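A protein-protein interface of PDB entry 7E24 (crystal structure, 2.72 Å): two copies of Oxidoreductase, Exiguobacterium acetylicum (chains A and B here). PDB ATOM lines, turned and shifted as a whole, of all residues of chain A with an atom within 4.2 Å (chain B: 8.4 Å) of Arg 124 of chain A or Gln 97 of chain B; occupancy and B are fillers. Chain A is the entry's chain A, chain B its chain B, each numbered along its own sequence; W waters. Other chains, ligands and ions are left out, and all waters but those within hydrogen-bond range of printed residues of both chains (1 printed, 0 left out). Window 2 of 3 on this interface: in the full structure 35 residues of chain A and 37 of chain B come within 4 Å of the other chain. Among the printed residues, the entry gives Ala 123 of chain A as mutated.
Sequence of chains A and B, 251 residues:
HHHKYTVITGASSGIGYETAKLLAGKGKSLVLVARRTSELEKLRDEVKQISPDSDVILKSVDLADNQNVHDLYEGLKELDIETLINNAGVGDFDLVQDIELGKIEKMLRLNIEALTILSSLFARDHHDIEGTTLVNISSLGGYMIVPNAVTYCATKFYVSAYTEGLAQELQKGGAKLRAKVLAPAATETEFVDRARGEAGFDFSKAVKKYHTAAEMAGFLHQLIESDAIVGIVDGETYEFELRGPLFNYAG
Printed residues of chain B within 4 Å of Ser 120 of chain A: Val 96 (3.9 Å) and Ile 99 (3.3 Å). Of chain B, only Gln 97 comes within 4 Å of Ala 123 of chain A. Of the printed residues of chain B, Arg 124 of chain A touches Gln 97. No residue of chain B comes within 4 Å of Asp 125 of chain A. Of the printed residues of chain B, His 127 of chain A touches Gln 97 (3.3 Å). Of the printed residues of chain A, Val 96 of chain B touches Ser 120. Of the printed residues of chain A, Gln 97 of chain B touches Ala 123 (3.8 Å), Arg 124 (3.5 Å) and His 127 (3.3 Å). Printed residues of chain A within 4 Å of Ile 99 of chain B: Ser 120 (3.3 Å). The nearest printed residue of chain B that does not touch Ser 120 of chain A is Leu 101 of chain B (4.02 Å).
The backbone carbonyl oxygen (O) of Ala 123 of chain A sits at hydrogen-bond distance from a ring nitrogen (ND1) of His 127 of chain A (3.3 Å). OD1 of Asp 125 of chain A lies within salt-bridge range of NE of Arg 124 of chain A (2.6 Å). O of Arg 124 of chain A lies within hydrogen-bond range of ND1 of His 127 of chain A (3.2 Å).
Water W1 bridges the backbone carbonyl oxygen of Val 96 of chain B and the backbone carbonyl oxygen of Ser 120 of chain A.
Hydrophobic or aromatic side chains of chain A within 4 Å of the printed part of chain B: His 127. Of the 10 printed residues of chain B, 3 touch a printed residue of chain A. Hydrophobic or aromatic side chains of chain B that line the printed part of chain A: Val 96 and Ile 99. Among the printed residues, no Asp or Glu carboxylate lies within 4 Å of a Lys or Arg side-chain nitrogen of the other chain.
No position is printed for both chains.
A ring nitrogen (NE2) of His 127 of chain A lies within hydrogen-bond range of the side-chain amide nitrogen (NE2) of Gln 97 of chain B, 3.3 Å away.
Among the printed residues, merely in contact across the chains: Ser 120 of chain A with Val 96 of chain B (3.9 Å), Ser 120 of chain A with Ile 99 of chain B (3.3 Å), Ala 123 of chain A with Gln 97 of chain B (3.8 Å) and Arg 124 of chain A with Gln 97 of chain B (3.5 Å).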
ATOM      1  N   SER A 120      27.149  19.732   0.626  1.00  0.00           N
ATOM      2  CA  SER A 120      26.620  18.519   1.231  1.00  0.00           C
ATOM      3  C   SER A 120      26.283  17.482   0.168  1.00  0.00           C
ATOM      4  O   SER A 120      26.583  16.296   0.336  1.00  0.00           O
ATOM      5  CB  SER A 120      25.394  18.856   2.063  1.00  0.00           C
ATOM      6  OG  SER A 120      25.714  19.809   3.057  1.00  0.00           O
ATOM      7  N   LEU A 121      25.688  17.915  -0.950  1.00  0.00           N
ATOM      8  CA  LEU A 121      25.308  16.966  -1.989  1.00  0.00           C
ATOM      9  C   LEU A 121      26.540  16.432  -2.699  1.00  0.00           C
ATOM     10  O   LEU A 121      26.658  15.221  -2.937  1.00  0.00           O
ATOM     11  CB  LEU A 121      24.336  17.618  -2.976  1.00  0.00           C
ATOM     12  CG  LEU A 121      22.913  17.877  -2.462  1.00  0.00           C
ATOM     13  CD1 LEU A 121      22.141  18.816  -3.371  1.00  0.00           C
ATOM     14  CD2 LEU A 121      22.152  16.583  -2.282  1.00  0.00           C
ATOM     15  N   PHE A 122      27.475  17.317  -3.030  1.00  0.00           N
ATOM     16  CA  PHE A 122      28.726  16.863  -3.612  1.00  0.00           C
ATOM     17  C   PHE A 122      29.423  15.874  -2.694  1.00  0.00           C
ATOM     18  O   PHE A 122      29.879  14.822  -3.142  1.00  0.00           O
ATOM     19  CB  PHE A 122      29.616  18.053  -3.904  1.00  0.00           C
ATOM     20  CG  PHE A 122      30.714  17.758  -4.849  1.00  0.00           C
ATOM     21  CD1 PHE A 122      30.445  17.371  -6.160  1.00  0.00           C
ATOM     22  CD2 PHE A 122      32.016  17.859  -4.436  1.00  0.00           C
ATOM     23  CE1 PHE A 122      31.471  17.099  -7.030  1.00  0.00           C
ATOM     24  CE2 PHE A 122      33.035  17.591  -5.296  1.00  0.00           C
ATOM     25  CZ  PHE A 122      32.771  17.206  -6.597  1.00  0.00           C
ATOM     26  N   ALA A 123      29.487  16.171  -1.391  1.00  0.00           N
ATOM     27  CA  ALA A 123      30.148  15.246  -0.476  1.00  0.00           C
ATOM     28  C   ALA A 123      29.400  13.921  -0.393  1.00  0.00           C
ATOM     29  O   ALA A 123      30.023  12.861  -0.300  1.00  0.00           O
ATOM     30  CB  ALA A 123      30.297  15.867   0.908  1.00  0.00           C
ATOM     31  N   ARG A 124      28.067  13.950  -0.449  1.00  0.00           N
ATOM     32  CA  ARG A 124      27.328  12.698  -0.349  1.00  0.00           C
ATOM     33  C   ARG A 124      27.743  11.739  -1.457  1.00  0.00           C
ATOM     34  O   ARG A 124      28.110  10.592  -1.186  1.00  0.00           O
ATOM     35  CB  ARG A 124      25.824  12.938  -0.382  1.00  0.00           C
ATOM     36  CG  ARG A 124      25.063  11.639  -0.175  1.00  0.00           C
ATOM     37  CD  ARG A 124      23.634  11.779  -0.604  1.00  0.00           C
ATOM     38  NE  ARG A 124      23.562  12.318  -1.959  1.00  0.00           N
ATOM     39  CZ  ARG A 124      22.509  12.973  -2.441  1.00  0.00           C
ATOM     40  NH1 ARG A 124      21.439  13.175  -1.677  1.00  0.00           N
ATOM     41  NH2 ARG A 124      22.527  13.439  -3.680  1.00  0.00           N
ATOM     42  N   ASP A 125      27.762  12.208  -2.712  1.00  0.00           N
ATOM     43  CA  ASP A 125      28.006  11.333  -3.859  1.00  0.00           C
ATOM     44  C   ASP A 125      29.467  11.217  -4.265  1.00  0.00           C
ATOM     45  O   ASP A 125      29.773  10.397  -5.132  1.00  0.00           O
ATOM     46  CB  ASP A 125      27.224  11.801  -5.087  1.00  0.00           C
ATOM     47  CG  ASP A 125      25.818  12.185  -4.754  1.00  0.00           C
ATOM     48  OD1 ASP A 125      25.291  11.631  -3.764  1.00  0.00           O
ATOM     49  OD2 ASP A 125      25.237  13.025  -5.469  1.00  0.00           O
ATOM     50  N   HIS A 126      30.381  11.992  -3.679  1.00  0.00           N
ATOM     51  CA  HIS A 126      31.736  12.040  -4.202  1.00  0.00           C
ATOM     52  C   HIS A 126      32.809  11.764  -3.168  1.00  0.00           C
ATOM     53  O   HIS A 126      33.995  11.868  -3.495  1.00  0.00           O
ATOM     54  CB  HIS A 126      32.025  13.397  -4.839  1.00  0.00           C
ATOM     55  CG  HIS A 126      31.204  13.687  -6.051  1.00  0.00           C
ATOM     56  ND1 HIS A 126      29.924  14.198  -5.989  1.00  0.00           N
ATOM     57  CD2 HIS A 126      31.488  13.543  -7.364  1.00  0.00           C
ATOM     58  CE1 HIS A 126      29.459  14.365  -7.213  1.00  0.00           C
ATOM     59  NE2 HIS A 126      30.387  13.970  -8.066  1.00  0.00           N
ATOM     60  N   HIS A 127      32.449  11.437  -1.928  1.00  0.00           N
ATOM     61  CA  HIS A 127      33.487  11.343  -0.910  1.00  0.00           C
ATOM     62  C   HIS A 127      34.465  10.212  -1.224  1.00  0.00           C
ATOM     63  O   HIS A 127      35.680  10.370  -1.049  1.00  0.00           O
ATOM     64  CB  HIS A 127      32.862  11.196   0.476  1.00  0.00           C
ATOM     65  CG  HIS A 127      32.162   9.901   0.676  1.00  0.00           C
ATOM     66  ND1 HIS A 127      30.849   9.719   0.309  1.00  0.00           N
ATOM     67  CD2 HIS A 127      32.582   8.721   1.193  1.00  0.00           C
ATOM     68  CE1 HIS A 127      30.485   8.481   0.590  1.00  0.00           C
ATOM     69  NE2 HIS A 127      31.518   7.854   1.128  1.00  0.00           N
ATOM     70  N   LEU A 170      36.833  14.672   6.280  1.00  0.00           N
ATOM     71  CA  LEU A 170      37.147  13.782   5.167  1.00  0.00           C
ATOM     72  C   LEU A 170      38.556  13.210   5.288  1.00  0.00           C
ATOM     73  O   LEU A 170      38.792  12.064   4.891  1.00  0.00           O
ATOM     74  CB  LEU A 170      36.986  14.538   3.856  1.00  0.00           C
ATOM     75  CG  LEU A 170      35.585  15.023   3.572  1.00  0.00           C
ATOM     76  CD1 LEU A 170      35.654  16.048   2.515  1.00  0.00           C
ATOM     77  CD2 LEU A 170      34.733  13.890   3.117  1.00  0.00           C
ATOM     78  N   ASP B  94      26.281  14.140  12.700  1.00  0.00           N
ATOM     79  CA  ASP B  94      26.340  13.359  11.464  1.00  0.00           C
ATOM     80  C   ASP B  94      27.507  13.802  10.591  1.00  0.00           C
ATOM     81  O   ASP B  94      27.821  14.994  10.554  1.00  0.00           O
ATOM     82  CB  ASP B  94      25.028  13.476  10.666  1.00  0.00           C
ATOM     83  CG  ASP B  94      24.176  12.191  10.708  1.00  0.00           C
ATOM     84  OD1 ASP B  94      24.723  11.102  10.974  1.00  0.00           O
ATOM     85  OD2 ASP B  94      22.955  12.261  10.437  1.00  0.00           O
ATOM     86  N   LEU B  95      28.170  12.860   9.914  1.00  0.00           N
ATOM     87  CA  LEU B  95      29.104  13.246   8.867  1.00  0.00           C
ATOM     88  C   LEU B  95      28.357  14.082   7.850  1.00  0.00           C
ATOM     89  O   LEU B  95      27.165  13.864   7.623  1.00  0.00           O
ATOM     90  CB  LEU B  95      29.694  12.018   8.192  1.00  0.00           C
ATOM     91  CG  LEU B  95      30.471  11.084   9.107  1.00  0.00           C
ATOM     92  CD1 LEU B  95      31.126   9.989   8.300  1.00  0.00           C
ATOM     93  CD2 LEU B  95      31.490  11.859   9.925  1.00  0.00           C
ATOM     94  N   VAL B  96      29.042  15.073   7.261  1.00  0.00           N
ATOM     95  CA  VAL B  96      28.356  15.922   6.286  1.00  0.00           C
ATOM     96  C   VAL B  96      27.776  15.075   5.156  1.00  0.00           C
ATOM     97  O   VAL B  96      26.639  15.293   4.713  1.00  0.00           O
ATOM     98  CB  VAL B  96      29.296  17.009   5.742  1.00  0.00           C
ATOM     99  CG1 VAL B  96      28.661  17.715   4.556  1.00  0.00           C
ATOM    100  CG2 VAL B  96      29.602  18.003   6.805  1.00  0.00           C
ATOM    101  N   GLN B  97      28.534  14.068   4.700  1.00  0.00           N
ATOM    102  CA  GLN B  97      28.052  13.154   3.673  1.00  0.00           C
ATOM    103  C   GLN B  97      26.781  12.405   4.081  1.00  0.00           C
ATOM    104  O   GLN B  97      26.096  11.855   3.208  1.00  0.00           O
ATOM    105  CB  GLN B  97      29.156  12.149   3.327  1.00  0.00           C
ATOM    106  CG  GLN B  97      29.566  11.252   4.464  1.00  0.00           C
ATOM    107  CD  GLN B  97      30.906  10.573   4.241  1.00  0.00           C
ATOM    108  OE1 GLN B  97      31.948  11.225   4.212  1.00  0.00           O
ATOM    109  NE2 GLN B  97      30.884   9.256   4.083  1.00  0.00           N
ATOM    110  N   ASP B  98      26.420  12.385   5.366  1.00  0.00           N
ATOM    111  CA  ASP B  98      25.251  11.631   5.791  1.00  0.00           C
ATOM    112  C   ASP B  98      24.077  12.502   6.203  1.00  0.00           C
ATOM    113  O   ASP B  98      23.048  11.961   6.628  1.00  0.00           O
ATOM    114  CB  ASP B  98      25.623  10.698   6.937  1.00  0.00           C
ATOM    115  CG  ASP B  98      26.545   9.563   6.482  1.00  0.00           C
ATOM    116  OD1 ASP B  98      26.550   9.276   5.271  1.00  0.00           O
ATOM    117  OD2 ASP B  98      27.246   8.943   7.320  1.00  0.00           O
ATOM    118  N   ILE B  99      24.167  13.826   6.075  1.00  0.00           N
ATOM    119  CA  ILE B  99      23.130  14.648   6.708  1.00  0.00           C
ATOM    120  C   ILE B  99      21.806  14.497   5.976  1.00  0.00           C
ATOM    121  O   ILE B  99      21.715  13.918   4.898  1.00  0.00           O
ATOM    122  CB  ILE B  99      23.535  16.128   6.779  1.00  0.00           C
ATOM    123  CG1 ILE B  99      23.764  16.662   5.369  1.00  0.00           C
ATOM    124  CG2 ILE B  99      24.720  16.343   7.717  1.00  0.00           C
ATOM    125  CD1 ILE B  99      23.888  18.142   5.268  1.00  0.00           C
ATOM    126  N   GLU B 100      20.767  15.026   6.606  1.00  0.00           N
ATOM    127  CA  GLU B 100      19.416  15.118   6.069  1.00  0.00           C
ATOM    128  C   GLU B 100      19.200  16.589   5.717  1.00  0.00           C
ATOM    129  O   GLU B 100      19.038  17.423   6.611  1.00  0.00           O
ATOM    130  CB  GLU B 100      18.401  14.638   7.117  1.00  0.00           C
ATOM    131  CG  GLU B 100      17.103  14.023   6.578  1.00  0.00           C
ATOM    132  CD  GLU B 100      16.113  15.059   6.059  1.00  0.00           C
ATOM    133  OE1 GLU B 100      15.697  15.908   6.884  1.00  0.00           O
ATOM    134  OE2 GLU B 100      15.744  15.010   4.851  1.00  0.00           O
ATOM    135  N   LEU B 101      19.253  16.930   4.430  1.00  0.00           N
ATOM    136  CA  LEU B 101      19.286  18.349   4.071  1.00  0.00           C
ATOM    137  C   LEU B 101      18.095  19.103   4.657  1.00  0.00           C
ATOM    138  O   LEU B 101      18.245  20.230   5.160  1.00  0.00           O
ATOM    139  CB  LEU B 101      19.333  18.525   2.551  1.00  0.00           C
ATOM    140  CG  LEU B 101      20.736  18.564   1.894  1.00  0.00           C
ATOM    141  CD1 LEU B 101      21.495  19.818   2.325  1.00  0.00           C
ATOM    142  CD2 LEU B 101      21.546  17.310   2.194  1.00  0.00           C
ATOM    143  N   VAL B 150      29.903  19.184  12.194  1.00  0.00           N
ATOM    144  CA  VAL B 150      30.548  20.237  11.422  1.00  0.00           C
ATOM    145  C   VAL B 150      29.557  21.350  11.122  1.00  0.00           C
ATOM    146  O   VAL B 150      29.800  22.531  11.415  1.00  0.00           O
ATOM    147  CB  VAL B 150      31.150  19.633  10.144  1.00  0.00           C
ATOM    148  CG1 VAL B 150      31.646  20.715   9.212  1.00  0.00           C
ATOM    149  CG2 VAL B 150      32.261  18.697  10.541  1.00  0.00           C
ATOM    150  N   THR B 151      28.396  20.975  10.586  1.00  0.00           N
ATOM    151  CA  THR B 151      27.409  21.937  10.111  1.00  0.00           C
ATOM    152  C   THR B 151      26.857  22.776  11.259  1.00  0.00           C
ATOM    153  O   THR B 151      26.706  24.001  11.142  1.00  0.00           O
ATOM    154  CB  THR B 151      26.296  21.170   9.388  1.00  0.00           C
ATOM    155  OG1 THR B 151      26.863  20.055   8.671  1.00  0.00           O
ATOM    156  CG2 THR B 151      25.529  22.078   8.436  1.00  0.00           C
HETATM  157  O   HOH W   1      25.121  15.292   2.529  1.00  0.00           O
